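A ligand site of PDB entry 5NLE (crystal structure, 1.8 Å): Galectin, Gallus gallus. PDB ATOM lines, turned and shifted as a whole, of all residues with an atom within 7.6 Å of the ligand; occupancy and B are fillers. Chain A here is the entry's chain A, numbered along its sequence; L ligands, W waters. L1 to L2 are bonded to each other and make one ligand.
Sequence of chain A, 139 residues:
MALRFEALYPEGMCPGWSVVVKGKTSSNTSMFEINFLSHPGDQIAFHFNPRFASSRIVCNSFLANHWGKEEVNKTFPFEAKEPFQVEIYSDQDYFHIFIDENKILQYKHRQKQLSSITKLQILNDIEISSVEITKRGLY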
ATOM      1  N   MET A  31      -2.427  19.382  11.755  1.00  0.00           N
ATOM      2  CA  MET A  31      -2.732  18.891  13.088  1.00  0.00           C
ATOM      3  C   MET A  31      -1.933  17.624  13.401  1.00  0.00           C
ATOM      4  O   MET A  31      -1.478  16.932  12.506  1.00  0.00           O
ATOM      5  CB  MET A  31      -4.226  18.632  13.241  1.00  0.00           C
ATOM      6  CG  MET A  31      -4.835  17.768  12.157  1.00  0.00           C
ATOM      7  SD  MET A  31      -5.847  16.482  12.890  1.00  0.00           S
ATOM      8  CE  MET A  31      -4.540  15.465  13.559  1.00  0.00           C
ATOM      9  N   GLU A  33      -1.603  14.338  16.687  1.00  0.00           N
ATOM     10  CA  GLU A  33      -2.206  13.839  17.896  1.00  0.00           C
ATOM     11  C   GLU A  33      -1.264  12.926  18.644  1.00  0.00           C
ATOM     12  O   GLU A  33      -0.400  12.276  18.055  1.00  0.00           O
ATOM     13  CB  GLU A  33      -3.527  13.120  17.591  1.00  0.00           C
ATOM     14  CG  GLU A  33      -3.461  12.090  16.501  1.00  0.00           C
ATOM     15  CD  GLU A  33      -4.855  11.579  16.112  1.00  0.00           C
ATOM     16  OE1 GLU A  33      -5.300  10.548  16.679  1.00  0.00           O
ATOM     17  OE2 GLU A  33      -5.510  12.215  15.247  1.00  0.00           O
ATOM     18  N   ASN A  35      -1.704   9.910  21.401  1.00  0.00           N
ATOM     19  CA  ASN A  35      -2.703   9.034  22.006  1.00  0.00           C
ATOM     20  C   ASN A  35      -2.077   8.119  23.060  1.00  0.00           C
ATOM     21  O   ASN A  35      -0.984   7.621  22.864  1.00  0.00           O
ATOM     22  CB  ASN A  35      -3.386   8.161  20.943  1.00  0.00           C
ATOM     23  CG  ASN A  35      -4.175   8.974  19.944  1.00  0.00           C
ATOM     24  OD1 ASN A  35      -4.775   9.984  20.286  1.00  0.00           O
ATOM     25  ND2 ASN A  35      -4.183   8.513  18.690  1.00  0.00           N
ATOM     26  N   HIS A  47      -6.563  11.256  24.236  1.00  0.00           N
ATOM     27  CA  HIS A  47      -6.318  11.717  22.875  1.00  0.00           C
ATOM     28  C   HIS A  47      -6.054  13.225  22.971  1.00  0.00           C
ATOM     29  O   HIS A  47      -6.936  13.986  23.389  1.00  0.00           O
ATOM     30  CB  HIS A  47      -7.552  11.410  22.013  1.00  0.00           C
ATOM     31  CG  HIS A  47      -7.557  12.037  20.652  1.00  0.00           C
ATOM     32  ND1 HIS A  47      -6.800  11.564  19.601  1.00  0.00           N
ATOM     33  CD2 HIS A  47      -8.300  13.050  20.139  1.00  0.00           C
ATOM     34  CE1 HIS A  47      -7.047  12.289  18.517  1.00  0.00           C
ATOM     35  NE2 HIS A  47      -7.966  13.182  18.822  1.00  0.00           N
ATOM     36  N   PHE A  48      -4.838  13.638  22.618  1.00  0.00           N
ATOM     37  CA  PHE A  48      -4.411  15.036  22.666  1.00  0.00           C
ATOM     38  C   PHE A  48      -4.239  15.514  21.239  1.00  0.00           C
ATOM     39  O   PHE A  48      -3.354  15.045  20.564  1.00  0.00           O
ATOM     40  CB  PHE A  48      -3.110  15.148  23.476  1.00  0.00           C
ATOM     41  CG  PHE A  48      -2.455  16.505  23.428  1.00  0.00           C
ATOM     42  CD1 PHE A  48      -2.835  17.520  24.310  1.00  0.00           C
ATOM     43  CD2 PHE A  48      -1.389  16.741  22.565  1.00  0.00           C
ATOM     44  CE1 PHE A  48      -2.212  18.751  24.277  1.00  0.00           C
ATOM     45  CE2 PHE A  48      -0.744  17.987  22.554  1.00  0.00           C
ATOM     46  CZ  PHE A  48      -1.164  18.985  23.406  1.00  0.00           C
ATOM     47  N   ASN A  49      -5.082  16.444  20.778  1.00  0.00           N
ATOM     48  CA  ASN A  49      -5.141  16.767  19.353  1.00  0.00           C
ATOM     49  C   ASN A  49      -5.094  18.269  19.076  1.00  0.00           C
ATOM     50  O   ASN A  49      -6.144  18.924  19.021  1.00  0.00           O
ATOM     51  CB  ASN A  49      -6.403  16.105  18.778  1.00  0.00           C
ATOM     52  CG  ASN A  49      -6.607  16.343  17.286  1.00  0.00           C
ATOM     53  OD1 ASN A  49      -7.770  16.378  16.826  1.00  0.00           O
ATOM     54  ND2 ASN A  49      -5.524  16.486  16.517  1.00  0.00           N
ATOM     55  N   ARG A  51      -5.081  21.274  16.796  1.00  0.00           N
ATOM     56  CA  ARG A  51      -5.545  21.543  15.450  1.00  0.00           C
ATOM     57  C   ARG A  51      -5.099  22.946  15.089  1.00  0.00           C
ATOM     58  O   ARG A  51      -5.589  23.912  15.667  1.00  0.00           O
ATOM     59  CB  ARG A  51      -7.071  21.380  15.371  1.00  0.00           C
ATOM     60  CG  ARG A  51      -7.513  19.935  15.689  1.00  0.00           C
ATOM     61  CD  ARG A  51      -9.032  19.789  15.734  1.00  0.00           C
ATOM     62  NE  ARG A  51      -9.405  18.439  16.162  1.00  0.00           N
ATOM     63  CZ  ARG A  51     -10.653  17.990  16.258  1.00  0.00           C
ATOM     64  NH1 ARG A  51     -11.666  18.792  15.948  1.00  0.00           N
ATOM     65  NH2 ARG A  51     -10.884  16.741  16.654  1.00  0.00           N
ATOM     66  N   ARG A  56      -7.060  25.307  18.148  1.00  0.00           N
ATOM     67  CA  ARG A  56      -7.700  24.668  19.294  1.00  0.00           C
ATOM     68  C   ARG A  56      -6.979  23.382  19.638  1.00  0.00           C
ATOM     69  O   ARG A  56      -6.555  22.655  18.749  1.00  0.00           O
ATOM     70  CB  ARG A  56      -9.172  24.322  19.016  1.00  0.00           C
ATOM     71  CG  ARG A  56     -10.063  25.445  18.494  1.00  0.00           C
ATOM     72  CD  ARG A  56     -11.510  24.927  18.344  1.00  0.00           C
ATOM     73  NE  ARG A  56     -11.617  23.770  17.459  1.00  0.00           N
ATOM     74  CZ  ARG A  56     -12.540  22.822  17.559  1.00  0.00           C
ATOM     75  NH1 ARG A  56     -13.462  22.873  18.515  1.00  0.00           N
ATOM     76  NH2 ARG A  56     -12.549  21.812  16.699  1.00  0.00           N
ATOM     77  N   VAL A  58      -7.966  19.864  21.071  1.00  0.00           N
ATOM     78  CA  VAL A  58      -9.087  19.010  21.424  1.00  0.00           C
ATOM     79  C   VAL A  58      -8.583  17.770  22.153  1.00  0.00           C
ATOM     80  O   VAL A  58      -7.701  17.086  21.637  1.00  0.00           O
ATOM     81  CB  VAL A  58      -9.885  18.578  20.186  1.00  0.00           C
ATOM     82  CG1 VAL A  58     -11.044  17.649  20.575  1.00  0.00           C
ATOM     83  CG2 VAL A  58     -10.397  19.796  19.431  1.00  0.00           C
ATOM     84  N   CYS A  59      -9.111  17.503  23.335  1.00  0.00           N
ATOM     85  CA  CYS A  59      -8.816  16.273  24.057  1.00  0.00           C
ATOM     86  C   CYS A  59     -10.069  15.433  24.230  1.00  0.00           C
ATOM     87  O   CYS A  59     -11.180  15.947  24.386  1.00  0.00           O
ATOM     88  CB  CYS A  59      -8.225  16.551  25.439  1.00  0.00           C
ATOM     89  SG  CYS A  59      -6.667  17.460  25.374  1.00  0.00           S
ATOM     90  N   ASN A  60      -9.879  14.125  24.212  1.00  0.00           N
ATOM     91  CA  ASN A  60     -11.025  13.257  24.333  1.00  0.00           C
ATOM     92  C   ASN A  60     -10.547  11.840  24.575  1.00  0.00           C
ATOM     93  O   ASN A  60      -9.350  11.604  24.716  1.00  0.00           O
ATOM     94  CB  ASN A  60     -11.889  13.370  23.067  1.00  0.00           C
ATOM     95  CG  ASN A  60     -13.322  12.931  23.298  1.00  0.00           C
ATOM     96  OD1 ASN A  60     -13.648  12.302  24.312  1.00  0.00           O
ATOM     97  ND2 ASN A  60     -14.196  13.238  22.349  1.00  0.00           N
ATOM     98  N   SER A  61     -11.496  10.907  24.653  1.00  0.00           N
ATOM     99  CA  SER A  61     -11.202   9.502  24.855  1.00  0.00           C
ATOM    100  C   SER A  61     -12.046   8.730  23.864  1.00  0.00           C
ATOM    101  O   SER A  61     -13.150   9.153  23.526  1.00  0.00           O
ATOM    102  CB  SER A  61     -11.496   9.058  26.293  1.00  0.00           C
ATOM    103  OG  SER A  61     -10.665   9.715  27.232  1.00  0.00           O
ATOM    104  N   PHE A  62     -11.510   7.623  23.380  1.00  0.00           N
ATOM    105  CA  PHE A  62     -12.222   6.790  22.415  1.00  0.00           C
ATOM    106  C   PHE A  62     -12.345   5.426  23.055  1.00  0.00           C
ATOM    107  O   PHE A  62     -11.449   4.589  22.949  1.00  0.00           O
ATOM    108  CB  PHE A  62     -11.484   6.716  21.067  1.00  0.00           C
ATOM    109  CG  PHE A  62     -12.234   5.954  19.987  1.00  0.00           C
ATOM    110  CD1 PHE A  62     -13.331   6.525  19.338  1.00  0.00           C
ATOM    111  CD2 PHE A  62     -11.827   4.700  19.596  1.00  0.00           C
ATOM    112  CE1 PHE A  62     -14.011   5.838  18.346  1.00  0.00           C
ATOM    113  CE2 PHE A  62     -12.504   3.993  18.605  1.00  0.00           C
ATOM    114  CZ  PHE A  62     -13.589   4.577  17.973  1.00  0.00           C
ATOM    115  N   TRP A  67     -16.193   8.138  20.547  1.00  0.00           N
ATOM    116  CA  TRP A  67     -15.603   9.342  21.136  1.00  0.00           C
ATOM    117  C   TRP A  67     -16.533   9.891  22.198  1.00  0.00           C
ATOM    118  O   TRP A  67     -17.753   9.949  21.976  1.00  0.00           O
ATOM    119  CB  TRP A  67     -15.344  10.394  20.068  1.00  0.00           C
ATOM    120  CG  TRP A  67     -14.223  10.040  19.174  1.00  0.00           C
ATOM    121  CD1 TRP A  67     -14.282   9.610  17.875  1.00  0.00           C
ATOM    122  CD2 TRP A  67     -12.833  10.094  19.518  1.00  0.00           C
ATOM    123  NE1 TRP A  67     -13.006   9.399  17.394  1.00  0.00           N
ATOM    124  CE2 TRP A  67     -12.101   9.674  18.381  1.00  0.00           C
ATOM    125  CE3 TRP A  67     -12.131  10.449  20.678  1.00  0.00           C
ATOM    126  CZ2 TRP A  67     -10.707   9.601  18.373  1.00  0.00           C
ATOM    127  CZ3 TRP A  67     -10.741  10.376  20.679  1.00  0.00           C
ATOM    128  CH2 TRP A  67     -10.047   9.960  19.525  1.00  0.00           C
ATOM    129  N   GLY A  68     -15.982  10.284  23.334  1.00  0.00           N
ATOM    130  CA  GLY A  68     -16.761  10.887  24.410  1.00  0.00           C
ATOM    131  C   GLY A  68     -16.940  12.380  24.240  1.00  0.00           C
ATOM    132  O   GLY A  68     -16.848  12.911  23.140  1.00  0.00           O
ATOM    133  N   LYS A  69     -17.202  13.079  25.344  1.00  0.00           N
ATOM    134  CA  LYS A  69     -17.353  14.512  25.305  1.00  0.00           C
ATOM    135  C   LYS A  69     -16.008  15.179  25.039  1.00  0.00           C
ATOM    136  O   LYS A  69     -15.027  14.896  25.719  1.00  0.00           O
ATOM    137  CB  LYS A  69     -17.939  15.031  26.621  1.00  0.00           C
ATOM    138  CG  LYS A  69     -19.386  14.602  26.879  1.00  0.00           C
ATOM    139  CD  LYS A  69     -20.353  15.364  25.997  1.00  0.00           C
ATOM    140  CE  LYS A  69     -20.329  16.849  26.335  1.00  0.00           C
ATOM    141  NZ  LYS A  69     -21.004  17.605  25.277  1.00  0.00           N
ATOM    142  N   GLU A  70     -15.967  16.073  24.067  1.00  0.00           N
ATOM    143  CA  GLU A  70     -14.746  16.823  23.800  1.00  0.00           C
ATOM    144  C   GLU A  70     -14.411  17.800  24.906  1.00  0.00           C
ATOM    145  O   GLU A  70     -15.302  18.445  25.460  1.00  0.00           O
ATOM    146  CB  GLU A  70     -14.853  17.579  22.472  1.00  0.00           C
ATOM    147  CG  GLU A  70     -14.801  16.673  21.269  1.00  0.00           C
ATOM    148  CD  GLU A  70     -14.745  17.433  19.972  1.00  0.00           C
ATOM    149  OE1 GLU A  70     -14.925  18.672  19.993  1.00  0.00           O
ATOM    150  OE2 GLU A  70     -14.527  16.781  18.925  1.00  0.00           O
ATOM    151  N   GLU A  71     -13.135  17.918  25.234  1.00  0.00           N
ATOM    152  CA  GLU A  71     -12.684  18.983  26.129  1.00  0.00           C
ATOM    153  C   GLU A  71     -11.734  19.823  25.326  1.00  0.00           C
ATOM    154  O   GLU A  71     -10.672  19.361  24.919  1.00  0.00           O
ATOM    155  CB  GLU A  71     -12.029  18.425  27.403  1.00  0.00           C
ATOM    156  CG  GLU A  71     -12.964  17.465  28.167  1.00  0.00           C
ATOM    157  CD  GLU A  71     -12.411  17.007  29.505  1.00  0.00           C
ATOM    158  OE1 GLU A  71     -11.501  17.668  30.052  1.00  0.00           O
ATOM    159  OE2 GLU A  71     -12.906  15.967  30.017  1.00  0.00           O
ATOM    160  N   VAL A  72     -12.138  21.068  25.082  1.00  0.00           N
ATOM    161  CA  VAL A  72     -11.384  21.925  24.167  1.00  0.00           C
ATOM    162  C   VAL A  72     -10.720  23.035  24.919  1.00  0.00           C
ATOM    163  O   VAL A  72     -11.351  23.727  25.713  1.00  0.00           O
ATOM    164  CB  VAL A  72     -12.300  22.524  23.085  1.00  0.00           C
ATOM    165  CG1 VAL A  72     -11.478  23.369  22.124  1.00  0.00           C
ATOM    166  CG2 VAL A  72     -13.040  21.415  22.353  1.00  0.00           C
ATOM    167  N   ASN A 124       0.242  11.908  12.443  1.00  0.00           N
ATOM    168  CA  ASN A 124      -0.028  13.044  11.554  1.00  0.00           C
ATOM    169  C   ASN A 124       1.070  14.122  11.536  1.00  0.00           C
ATOM    170  O   ASN A 124       2.258  13.788  11.561  1.00  0.00           O
ATOM    171  CB  ASN A 124      -1.407  13.618  11.886  1.00  0.00           C
ATOM    172  CG  ASN A 124      -2.534  12.594  11.607  1.00  0.00           C
ATOM    173  OD1 ASN A 124      -3.527  12.503  12.330  1.00  0.00           O
ATOM    174  ND2 ASN A 124      -2.331  11.789  10.573  1.00  0.00           N
HETATM  175  C1  LIG L   1     -17.405  17.019  14.916  1.00  0.00           C
HETATM  176  C2  LIG L   1     -16.326  17.598  15.801  1.00  0.00           C
HETATM  177  C3  LIG L   1     -15.005  17.027  15.498  1.00  0.00           C
HETATM  178  C4  LIG L   1     -15.004  15.530  15.499  1.00  0.00           C
HETATM  179  C5  LIG L   1     -16.159  14.935  14.712  1.00  0.00           C
HETATM  180  C6  LIG L   1     -16.316  13.459  15.027  1.00  0.00           C
HETATM  181  O1  LIG L   1     -17.141  17.363  13.605  1.00  0.00           O
HETATM  182  O2  LIG L   1     -16.269  19.012  15.582  1.00  0.00           O
HETATM  183  O3  LIG L   1     -14.093  17.516  16.514  1.00  0.00           O
HETATM  184  O4  LIG L   1     -13.735  15.091  14.923  1.00  0.00           O
HETATM  185  O5  LIG L   1     -17.444  15.542  15.021  1.00  0.00           O
HETATM  186  O6  LIG L   1     -15.692  12.725  13.998  1.00  0.00           O
HETATM  187  C1  LG2 L   2     -13.142  14.086  15.664  1.00  0.00           C
HETATM  188  C2  LG2 L   2     -11.889  13.588  14.947  1.00  0.00           C
HETATM  189  C3  LG2 L   2     -11.156  12.576  15.752  1.00  0.00           C
HETATM  190  C4  LG2 L   2     -10.898  13.039  17.140  1.00  0.00           C
HETATM  191  C5  LG2 L   2     -12.201  13.486  17.790  1.00  0.00           C
HETATM  192  C6  LG2 L   2     -11.992  13.973  19.201  1.00  0.00           C
HETATM  193  O1  LG2 L   2     -12.315  13.017  13.699  1.00  0.00           O
HETATM  194  O2  LG2 L   2      -9.858  12.271  15.136  1.00  0.00           O
HETATM  195  O3  LG2 L   2      -9.953  14.103  17.097  1.00  0.00           O
HETATM  196  O4  LG2 L   2     -12.821  14.536  17.015  1.00  0.00           O
HETATM  197  O5  LG2 L   2     -13.247  14.343  19.750  1.00  0.00           O
HETATM  198  O   HOH W   1      -7.931  14.070  15.014  1.00  0.00           O
HETATM  199  O   HOH W   2     -16.390  14.243  19.050  1.00  0.00           O
HETATM  200  O   HOH W   3     -15.134  20.250  17.934  1.00  0.00           O
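An oxygen (O3) of LG2 L2 is in hydrogen-bond range of the side-chain amide oxygen of Asn 49, 3.2 Å away.
O3 of LG2 L2 is in hydrogen-bond range of NE2 of His 47 (2.8 Å).
The side-chain carboxylate (OE2) of Glu 70 is in hydrogen-bond range of an oxygen (O3) of LIG L1.
The side-chain amide nitrogen (ND2) of Asn 60 is in hydrogen-bond range of an oxygen (O5) of LG2 L2.
An oxygen (O3) of LIG L1 is in hydrogen-bond range of the guanidinium group of Arg 51, at 2.8 Å.
Water W1 lies within hydrogen-bond range of O2 of LG2 L2 (2.6 Å), OD1 of Asn 49 (2.9 Å) and OE2 of Glu 33 (3.1 Å).
Water W3 lies within hydrogen-bond range of the side-chain carboxylate (OE1) of Glu 70, an oxygen (O2) of LIG L1 and the guanidinium group (NH1) of Arg 56.
Water W2 bridges OE2 of Glu 70 (3.2 Å) and O5 of LG2 L2 (3.2 Å).
A ring nitrogen (ND1) of His 47 lies close to the side-chain carboxylate (OE1) of Glu 33 (3.4 Å).
The backbone carbonyl oxygen of Arg 56 sits at hydrogen-bond distance from the backbone NH of Arg 51, at 2.8 Å.
N of His 47 lies within hydrogen-bond range of O of Asn 60, 2.8 Å away.
The guanidinium group (NE) of Arg 51 sits at hydrogen-bond distance from the side-chain amide oxygen (OD1) of Asn 49 (2.7 Å).
ND2 of Asn 49 lies close to SD of Met 31 (3.6 Å).
OD1 of Asn 60 sits close to O of Lys 69 (3.3 Å).
A ring nitrogen (ND1) of His 47 lies within hydrogen-bond range of the side-chain amide oxygen (OD1) of Asn 35.
The backbone NH (N) of Asn 49 sits at hydrogen-bond distance from the backbone carbonyl oxygen (O) of Val 58 (2.8 Å).
Merely in contact with the ligand: Trp 67 (3.7 Å).
Hydrophobic or aromatic side chains within 4 Å of the ligand: His 47 and Trp 67.
Along chain A the residues within 4 Å of the ligand span positions 47 to 70.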
